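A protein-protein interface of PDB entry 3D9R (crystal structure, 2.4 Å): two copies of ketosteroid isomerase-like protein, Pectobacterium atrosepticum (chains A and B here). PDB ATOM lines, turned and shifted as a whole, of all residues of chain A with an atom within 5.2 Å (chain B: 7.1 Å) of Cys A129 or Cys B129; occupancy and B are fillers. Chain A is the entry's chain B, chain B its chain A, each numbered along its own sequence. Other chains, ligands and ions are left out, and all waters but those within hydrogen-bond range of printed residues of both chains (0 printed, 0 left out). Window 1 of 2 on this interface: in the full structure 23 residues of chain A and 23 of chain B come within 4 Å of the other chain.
Gln B110 touches Met A43 (CD to CB, 3.9 Å).
Met A43 touches Glu B111.
CE of Met A43 touches N of Leu B112, at 3.2 Å.
OE1 of Gln A110 touches CG of Met B43 (3.6 Å).
Glu A111 touches Met B43.
CB of Leu A112 touches CE of Met B43, at 3.7 Å.
Thr A130 touches Ser B131 (O to CB, 3.9 Å).
Ser A131 touches Gly B44 (OG to C, 3.2 Å).
O of Gly B44 is in hydrogen-bond range of NE2 of Gln A110 (3.1 Å).
The backbone nitrogen of Pro B45 sits close to the side-chain hydroxyl of Ser A131, at 3.1 Å.
SG of Cys B129 is in hydrogen-bond range of SG of Cys A129.
The backbone carbonyl oxygen (O) of Thr B130 sits at hydrogen-bond distance from the side-chain hydroxyl (OG) of Ser A131 (3.1 Å).
Met A43 touches Gln B110, and with the chains exchanged Gln A110 touches Met B43.
Met A43 touches Glu B111, and with the chains exchanged Glu A111 touches Met B43.
Cys A129 touches its own counterpart, Cys B129.
Thr A130 touches Ser B131, and with the chains exchanged Ser A131 touches Thr B130.
Of the 12 pairs that touch across the chains among the printed residues, 9 have their exchanged pair printed and touching as well.
Printed residues of chain A that touch a printed residue of chain B: Met A43, Gln A110, Glu A111, Leu A112, Cys A129, Thr A130 and Ser A131.
Hydrophobic or aromatic side chains of chain A within 4 Å of the printed part of chain B: Met A43 and Leu A112.
Of the 17 printed residues of chain B, 9 touch a printed residue of chain A.
Hydrophobic or aromatic side chains of chain B within 4 Å of the printed part of chain A: Met B43, Pro B45 and Leu B112.
Along chain B the printed residues that touch a printed residue of chain A span positions 43 to 131.
Among the printed residues, 12 pairs touch across the chains.
O of Gln A110 lies within hydrogen-bond range of N of Ser A131, 3.0 Å away.
NE2 of Gln B110 is in hydrogen-bond range of OG of Ser B131 (2.8 Å).
The backbone NH (N) of Leu A112 lies within hydrogen-bond range of the backbone carbonyl oxygen (O) of Cys A129 (2.9 Å).
O of Met B43 lies within hydrogen-bond range of N of Thr B130 (2.9 Å).
O of Cys B129 sits at hydrogen-bond distance from N of Leu B112 (2.9 Å).
N of Met A43 lies within hydrogen-bond range of O of Tyr A128, at 2.9 Å.
Of the printed residues of chain B, Cys A129 touches Cys B129 (3.2 Å).
Of the printed residues of chain A, Thr B130 touches Ser A131.
Of the printed residues of chain B, Ser A131 touches Gly B44, Pro B45 and Thr B130.
Printed residues of chain A within 4 Å of Met B43: Gln A110, Glu A111 and Leu A112.
Printed residues of chain A within 4 Å of Glu B111: Met A43.
Printed residues of chain A within 4 Å of Gly B44: Gln A110 and Ser A131.
The nearest printed residue of chain B that does not touch Cys A129 is Ser B131 (4.5 Å).
The nearest printed residue of chain A that does not touch Cys B129 is Leu A112 (4.4 Å).
The nearest printed residue of chain A that does not touch Glu B111 is Cys A129 (5.7 Å).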
ATOM      1  N   MET A  43      -4.714  25.721 -15.534  1.00  0.00           N
ATOM      2  CA  MET A  43      -5.331  24.602 -16.208  1.00  0.00           C
ATOM      3  C   MET A  43      -6.319  23.990 -15.222  1.00  0.00           C
ATOM      4  O   MET A  43      -5.915  23.403 -14.215  1.00  0.00           O
ATOM      5  CB  MET A  43      -4.252  23.608 -16.605  1.00  0.00           C
ATOM      6  CG  MET A  43      -3.176  24.215 -17.517  1.00  0.00           C
ATOM      7  SD  MET A  43      -1.404  23.423 -17.316  1.00  0.00           S
ATOM      8  CE  MET A  43      -1.890  21.551 -17.510  1.00  0.00           C
ATOM      9  N   GLN A 110      -7.362  18.254  -6.462  1.00  0.00           N
ATOM     10  CA  GLN A 110      -5.937  18.058  -6.234  1.00  0.00           C
ATOM     11  C   GLN A 110      -5.231  19.020  -7.169  1.00  0.00           C
ATOM     12  O   GLN A 110      -5.691  19.265  -8.282  1.00  0.00           O
ATOM     13  CB  GLN A 110      -5.534  16.600  -6.491  1.00  0.00           C
ATOM     14  CG  GLN A 110      -5.869  16.088  -7.898  1.00  0.00           C
ATOM     15  CD  GLN A 110      -6.032  14.579  -7.974  1.00  0.00           C
ATOM     16  OE1 GLN A 110      -5.392  13.839  -7.231  1.00  0.00           O
ATOM     17  NE2 GLN A 110      -6.924  14.124  -8.856  1.00  0.00           N
ATOM     18  N   GLU A 111      -4.137  19.594  -6.693  1.00  0.00           N
ATOM     19  CA  GLU A 111      -3.493  20.727  -7.330  1.00  0.00           C
ATOM     20  C   GLU A 111      -1.995  20.528  -7.444  1.00  0.00           C
ATOM     21  O   GLU A 111      -1.377  19.986  -6.532  1.00  0.00           O
ATOM     22  CB  GLU A 111      -3.729  21.983  -6.473  1.00  0.00           C
ATOM     23  CG  GLU A 111      -5.171  22.392  -6.311  1.00  0.00           C
ATOM     24  CD  GLU A 111      -5.827  21.949  -5.024  1.00  0.00           C
ATOM     25  OE1 GLU A 111      -5.126  21.721  -4.009  1.00  0.00           O
ATOM     26  OE2 GLU A 111      -7.078  21.889  -5.020  1.00  0.00           O
ATOM     27  N   LEU A 112      -1.409  20.996  -8.546  1.00  0.00           N
ATOM     28  CA  LEU A 112       0.054  21.061  -8.710  1.00  0.00           C
ATOM     29  C   LEU A 112       0.424  22.509  -8.969  1.00  0.00           C
ATOM     30  O   LEU A 112      -0.114  23.104  -9.868  1.00  0.00           O
ATOM     31  CB  LEU A 112       0.521  20.199  -9.887  1.00  0.00           C
ATOM     32  CG  LEU A 112       2.029  20.028 -10.167  1.00  0.00           C
ATOM     33  CD1 LEU A 112       2.764  19.411  -8.952  1.00  0.00           C
ATOM     34  CD2 LEU A 112       2.277  19.170 -11.422  1.00  0.00           C
ATOM     35  N   ARG A 127       2.971  28.117 -13.321  1.00  0.00           N
ATOM     36  CA  ARG A 127       1.982  27.208 -13.914  1.00  0.00           C
ATOM     37  C   ARG A 127       1.199  26.510 -12.808  1.00  0.00           C
ATOM     38  O   ARG A 127       1.788  26.106 -11.803  1.00  0.00           O
ATOM     39  CB  ARG A 127       2.682  26.120 -14.736  1.00  0.00           C
ATOM     40  CG  ARG A 127       3.576  26.601 -15.866  1.00  0.00           C
ATOM     41  CD  ARG A 127       2.822  27.320 -16.952  1.00  0.00           C
ATOM     42  NE  ARG A 127       3.748  27.906 -17.920  1.00  0.00           N
ATOM     43  CZ  ARG A 127       4.395  29.073 -17.786  1.00  0.00           C
ATOM     44  NH1 ARG A 127       4.277  29.816 -16.706  1.00  0.00           N
ATOM     45  NH2 ARG A 127       5.201  29.487 -18.756  1.00  0.00           N
ATOM     46  N   TYR A 128      -0.108  26.341 -12.998  1.00  0.00           N
ATOM     47  CA  TYR A 128      -0.956  25.692 -11.993  1.00  0.00           C
ATOM     48  C   TYR A 128      -1.996  24.814 -12.621  1.00  0.00           C
ATOM     49  O   TYR A 128      -2.688  25.251 -13.532  1.00  0.00           O
ATOM     50  CB  TYR A 128      -1.665  26.758 -11.185  1.00  0.00           C
ATOM     51  CG  TYR A 128      -2.686  26.266 -10.183  1.00  0.00           C
ATOM     52  CD1 TYR A 128      -2.306  25.698  -8.981  1.00  0.00           C
ATOM     53  CD2 TYR A 128      -4.032  26.456 -10.410  1.00  0.00           C
ATOM     54  CE1 TYR A 128      -3.252  25.298  -8.045  1.00  0.00           C
ATOM     55  CE2 TYR A 128      -4.976  26.061  -9.480  1.00  0.00           C
ATOM     56  CZ  TYR A 128      -4.580  25.493  -8.308  1.00  0.00           C
ATOM     57  OH  TYR A 128      -5.551  25.104  -7.434  1.00  0.00           O
ATOM     58  N   CYS A 129      -2.110  23.576 -12.148  1.00  0.00           N
ATOM     59  CA  CYS A 129      -3.101  22.638 -12.657  1.00  0.00           C
ATOM     60  C   CYS A 129      -3.946  22.149 -11.484  1.00  0.00           C
ATOM     61  O   CYS A 129      -3.396  21.830 -10.447  1.00  0.00           O
ATOM     62  CB  CYS A 129      -2.396  21.474 -13.361  1.00  0.00           C
ATOM     63  SG  CYS A 129      -3.358  20.627 -14.616  1.00  0.00           S
ATOM     64  N   THR A 130      -5.262  22.108 -11.672  1.00  0.00           N
ATOM     65  CA  THR A 130      -6.180  21.552 -10.699  1.00  0.00           C
ATOM     66  C   THR A 130      -7.104  20.568 -11.421  1.00  0.00           C
ATOM     67  O   THR A 130      -7.606  20.873 -12.482  1.00  0.00           O
ATOM     68  CB  THR A 130      -6.995  22.635  -9.991  1.00  0.00           C
ATOM     69  OG1 THR A 130      -7.868  22.017  -9.053  1.00  0.00           O
ATOM     70  CG2 THR A 130      -7.821  23.478 -10.976  1.00  0.00           C
ATOM     71  N   SER A 131      -7.282  19.385 -10.839  1.00  0.00           N
ATOM     72  CA  SER A 131      -8.150  18.341 -11.372  1.00  0.00           C
ATOM     73  C   SER A 131      -9.215  17.998 -10.327  1.00  0.00           C
ATOM     74  O   SER A 131      -8.935  18.000  -9.136  1.00  0.00           O
ATOM     75  CB  SER A 131      -7.312  17.100 -11.703  1.00  0.00           C
ATOM     76  OG  SER A 131      -7.962  16.284 -12.662  1.00  0.00           O
ATOM     77  N   TYR B  36       7.722   7.230 -16.529  1.00  0.00           N
ATOM     78  CA  TYR B  36       7.674   7.853 -15.201  1.00  0.00           C
ATOM     79  C   TYR B  36       8.908   7.513 -14.353  1.00  0.00           C
ATOM     80  O   TYR B  36       9.512   6.444 -14.502  1.00  0.00           O
ATOM     81  CB  TYR B  36       6.431   7.382 -14.434  1.00  0.00           C
ATOM     82  CG  TYR B  36       5.126   8.049 -14.798  1.00  0.00           C
ATOM     83  CD1 TYR B  36       4.743   9.241 -14.182  1.00  0.00           C
ATOM     84  CD2 TYR B  36       4.243   7.471 -15.725  1.00  0.00           C
ATOM     85  CE1 TYR B  36       3.529   9.874 -14.512  1.00  0.00           C
ATOM     86  CE2 TYR B  36       3.011   8.100 -16.056  1.00  0.00           C
ATOM     87  CZ  TYR B  36       2.669   9.291 -15.442  1.00  0.00           C
ATOM     88  OH  TYR B  36       1.470   9.914 -15.710  1.00  0.00           O
ATOM     89  N   VAL B  41       4.044  10.673  -9.928  1.00  0.00           N
ATOM     90  CA  VAL B  41       2.665  10.966  -9.551  1.00  0.00           C
ATOM     91  C   VAL B  41       1.811  11.322 -10.780  1.00  0.00           C
ATOM     92  O   VAL B  41       2.200  12.164 -11.611  1.00  0.00           O
ATOM     93  CB  VAL B  41       2.588  12.112  -8.507  1.00  0.00           C
ATOM     94  CG1 VAL B  41       1.200  12.207  -7.893  1.00  0.00           C
ATOM     95  CG2 VAL B  41       3.627  11.912  -7.432  1.00  0.00           C
ATOM     96  N   LEU B  42       0.659  10.649 -10.903  1.00  0.00           N
ATOM     97  CA  LEU B  42      -0.382  11.027 -11.855  1.00  0.00           C
ATOM     98  C   LEU B  42      -1.553  11.645 -11.117  1.00  0.00           C
ATOM     99  O   LEU B  42      -2.104  11.059 -10.175  1.00  0.00           O
ATOM    100  CB  LEU B  42      -0.838   9.819 -12.680  1.00  0.00           C
ATOM    101  CG  LEU B  42      -2.163   9.882 -13.484  1.00  0.00           C
ATOM    102  CD1 LEU B  42      -2.098  10.708 -14.776  1.00  0.00           C
ATOM    103  CD2 LEU B  42      -2.571   8.485 -13.818  1.00  0.00           C
ATOM    104  N   MET B  43      -1.914  12.848 -11.554  1.00  0.00           N
ATOM    105  CA  MET B  43      -3.128  13.527 -11.104  1.00  0.00           C
ATOM    106  C   MET B  43      -4.039  13.714 -12.308  1.00  0.00           C
ATOM    107  O   MET B  43      -3.698  14.390 -13.265  1.00  0.00           O
ATOM    108  CB  MET B  43      -2.811  14.871 -10.470  1.00  0.00           C
ATOM    109  CG  MET B  43      -2.382  14.780  -9.010  1.00  0.00           C
ATOM    110  SD  MET B  43      -1.796  16.507  -8.369  1.00  0.00           S
ATOM    111  CE  MET B  43      -0.133  16.611  -9.392  1.00  0.00           C
ATOM    112  N   GLY B  44      -5.195  13.057 -12.264  1.00  0.00           N
ATOM    113  CA  GLY B  44      -6.136  13.032 -13.367  1.00  0.00           C
ATOM    114  C   GLY B  44      -7.542  13.098 -12.805  1.00  0.00           C
ATOM    115  O   GLY B  44      -7.739  12.912 -11.604  1.00  0.00           O
ATOM    116  N   PRO B  45      -8.533  13.373 -13.661  1.00  0.00           N
ATOM    117  CA  PRO B  45      -9.883  13.609 -13.123  1.00  0.00           C
ATOM    118  C   PRO B  45     -10.586  12.331 -12.641  1.00  0.00           C
ATOM    119  O   PRO B  45     -10.330  11.236 -13.157  1.00  0.00           O
ATOM    120  CB  PRO B  45     -10.626  14.270 -14.298  1.00  0.00           C
ATOM    121  CG  PRO B  45      -9.537  14.546 -15.375  1.00  0.00           C
ATOM    122  CD  PRO B  45      -8.494  13.497 -15.129  1.00  0.00           C
ATOM    123  N   GLN B 110      -5.951  18.940 -21.216  1.00  0.00           N
ATOM    124  CA  GLN B 110      -4.735  19.731 -21.156  1.00  0.00           C
ATOM    125  C   GLN B 110      -3.856  19.125 -20.079  1.00  0.00           C
ATOM    126  O   GLN B 110      -4.347  18.667 -19.046  1.00  0.00           O
ATOM    127  CB  GLN B 110      -5.030  21.205 -20.889  1.00  0.00           C
ATOM    128  CG  GLN B 110      -5.796  21.455 -19.587  1.00  0.00           C
ATOM    129  CD  GLN B 110      -6.571  22.750 -19.590  1.00  0.00           C
ATOM    130  OE1 GLN B 110      -6.213  23.705 -20.299  1.00  0.00           O
ATOM    131  NE2 GLN B 110      -7.651  22.795 -18.801  1.00  0.00           N
ATOM    132  N   GLU B 111      -2.553  19.127 -20.342  1.00  0.00           N
ATOM    133  CA  GLU B 111      -1.582  18.372 -19.579  1.00  0.00           C
ATOM    134  C   GLU B 111      -0.336  19.172 -19.191  1.00  0.00           C
ATOM    135  O   GLU B 111       0.238  19.874 -20.025  1.00  0.00           O
ATOM    136  CB  GLU B 111      -1.139  17.182 -20.422  1.00  0.00           C
ATOM    137  CG  GLU B 111      -2.274  16.250 -20.789  1.00  0.00           C
ATOM    138  CD  GLU B 111      -2.701  16.307 -22.219  1.00  0.00           C
ATOM    139  OE1 GLU B 111      -1.967  16.842 -23.070  1.00  0.00           O
ATOM    140  OE2 GLU B 111      -3.792  15.777 -22.484  1.00  0.00           O
ATOM    141  N   LEU B 112       0.099  19.021 -17.936  1.00  0.00           N
ATOM    142  CA  LEU B 112       1.398  19.541 -17.480  1.00  0.00           C
ATOM    143  C   LEU B 112       2.297  18.373 -17.027  1.00  0.00           C
ATOM    144  O   LEU B 112       1.916  17.591 -16.141  1.00  0.00           O
ATOM    145  CB  LEU B 112       1.218  20.537 -16.332  1.00  0.00           C
ATOM    146  CG  LEU B 112       2.437  21.295 -15.787  1.00  0.00           C
ATOM    147  CD1 LEU B 112       3.057  22.191 -16.847  1.00  0.00           C
ATOM    148  CD2 LEU B 112       2.073  22.140 -14.532  1.00  0.00           C
ATOM    149  N   PHE B 113       3.467  18.281 -17.664  1.00  0.00           N
ATOM    150  CA  PHE B 113       4.549  17.385 -17.274  1.00  0.00           C
ATOM    151  C   PHE B 113       5.614  18.146 -16.523  1.00  0.00           C
ATOM    152  O   PHE B 113       6.059  19.187 -16.982  1.00  0.00           O
ATOM    153  CB  PHE B 113       5.291  16.804 -18.491  1.00  0.00           C
ATOM    154  CG  PHE B 113       4.442  16.050 -19.438  1.00  0.00           C
ATOM    155  CD1 PHE B 113       3.643  16.717 -20.362  1.00  0.00           C
ATOM    156  CD2 PHE B 113       4.499  14.662 -19.480  1.00  0.00           C
ATOM    157  CE1 PHE B 113       2.874  16.009 -21.268  1.00  0.00           C
ATOM    158  CE2 PHE B 113       3.750  13.963 -20.412  1.00  0.00           C
ATOM    159  CZ  PHE B 113       2.930  14.652 -21.297  1.00  0.00           C
ATOM    160  N   LEU B 114       6.053  17.582 -15.401  1.00  0.00           N
ATOM    161  CA  LEU B 114       7.301  17.949 -14.742  1.00  0.00           C
ATOM    162  C   LEU B 114       8.279  16.798 -14.939  1.00  0.00           C
ATOM    163  O   LEU B 114       8.101  15.720 -14.395  1.00  0.00           O
ATOM    164  CB  LEU B 114       7.086  18.179 -13.259  1.00  0.00           C
ATOM    165  CG  LEU B 114       6.932  19.594 -12.714  1.00  0.00           C
ATOM    166  CD1 LEU B 114       6.014  20.484 -13.568  1.00  0.00           C
ATOM    167  CD2 LEU B 114       6.427  19.496 -11.268  1.00  0.00           C
ATOM    168  N   THR B 125       9.135  11.591 -16.510  1.00  0.00           N
ATOM    169  CA  THR B 125       8.066  12.354 -15.882  1.00  0.00           C
ATOM    170  C   THR B 125       8.066  12.092 -14.380  1.00  0.00           C
ATOM    171  O   THR B 125       7.890  10.958 -13.944  1.00  0.00           O
ATOM    172  CB  THR B 125       6.698  11.926 -16.423  1.00  0.00           C
ATOM    173  OG1 THR B 125       6.700  11.989 -17.846  1.00  0.00           O
ATOM    174  CG2 THR B 125       5.602  12.805 -15.887  1.00  0.00           C
ATOM    175  N   ARG B 127       6.158  14.313 -12.219  1.00  0.00           N
ATOM    176  CA  ARG B 127       4.820  14.734 -11.786  1.00  0.00           C
ATOM    177  C   ARG B 127       4.022  15.056 -13.023  1.00  0.00           C
ATOM    178  O   ARG B 127       4.539  15.719 -13.934  1.00  0.00           O
ATOM    179  CB  ARG B 127       4.883  15.992 -10.890  1.00  0.00           C
ATOM    180  CG  ARG B 127       5.624  15.853  -9.573  1.00  0.00           C
ATOM    181  CD  ARG B 127       5.076  14.724  -8.669  1.00  0.00           C
ATOM    182  NE  ARG B 127       5.888  14.628  -7.466  1.00  0.00           N
ATOM    183  CZ  ARG B 127       7.034  13.962  -7.362  1.00  0.00           C
ATOM    184  NH1 ARG B 127       7.543  13.279  -8.378  1.00  0.00           N
ATOM    185  NH2 ARG B 127       7.689  14.002  -6.224  1.00  0.00           N
ATOM    186  N   TYR B 128       2.784  14.561 -13.077  1.00  0.00           N
ATOM    187  CA  TYR B 128       1.927  14.782 -14.243  1.00  0.00           C
ATOM    188  C   TYR B 128       0.482  15.069 -13.834  1.00  0.00           C
ATOM    189  O   TYR B 128      -0.081  14.349 -13.034  1.00  0.00           O
ATOM    190  CB  TYR B 128       2.013  13.560 -15.181  1.00  0.00           C
ATOM    191  CG  TYR B 128       1.102  13.585 -16.418  1.00  0.00           C
ATOM    192  CD1 TYR B 128       1.454  14.302 -17.541  1.00  0.00           C
ATOM    193  CD2 TYR B 128      -0.075  12.869 -16.453  1.00  0.00           C
ATOM    194  CE1 TYR B 128       0.658  14.316 -18.663  1.00  0.00           C
ATOM    195  CE2 TYR B 128      -0.887  12.882 -17.561  1.00  0.00           C
ATOM    196  CZ  TYR B 128      -0.519  13.606 -18.674  1.00  0.00           C
ATOM    197  OH  TYR B 128      -1.293  13.620 -19.826  1.00  0.00           O
ATOM    198  N   CYS B 129      -0.076  16.141 -14.391  1.00  0.00           N
ATOM    199  CA  CYS B 129      -1.450  16.577 -14.153  1.00  0.00           C
ATOM    200  C   CYS B 129      -2.175  16.640 -15.498  1.00  0.00           C
ATOM    201  O   CYS B 129      -1.637  17.199 -16.455  1.00  0.00           O
ATOM    202  CB  CYS B 129      -1.419  17.972 -13.512  1.00  0.00           C
ATOM    203  SG  CYS B 129      -2.739  18.382 -12.353  1.00  0.00           S
ATOM    204  N   THR B 130      -3.380  16.090 -15.558  1.00  0.00           N
ATOM    205  CA  THR B 130      -4.231  16.229 -16.723  1.00  0.00           C
ATOM    206  C   THR B 130      -5.618  16.720 -16.255  1.00  0.00           C
ATOM    207  O   THR B 130      -6.090  16.335 -15.186  1.00  0.00           O
ATOM    208  CB  THR B 130      -4.256  14.950 -17.567  1.00  0.00           C
ATOM    209  OG1 THR B 130      -5.007  15.205 -18.749  1.00  0.00           O
ATOM    210  CG2 THR B 130      -4.843  13.808 -16.825  1.00  0.00           C
ATOM    211  N   SER B 131      -6.201  17.655 -17.004  1.00  0.00           N
ATOM    212  CA  SER B 131      -7.521  18.189 -16.684  1.00  0.00           C
ATOM    213  C   SER B 131      -8.359  18.141 -17.942  1.00  0.00           C
ATOM    214  O   SER B 131      -7.854  18.380 -19.033  1.00  0.00           O
ATOM    215  CB  SER B 131      -7.428  19.622 -16.120  1.00  0.00           C
ATOM    216  OG  SER B 131      -7.448  20.611 -17.131  1.00  0.00           O
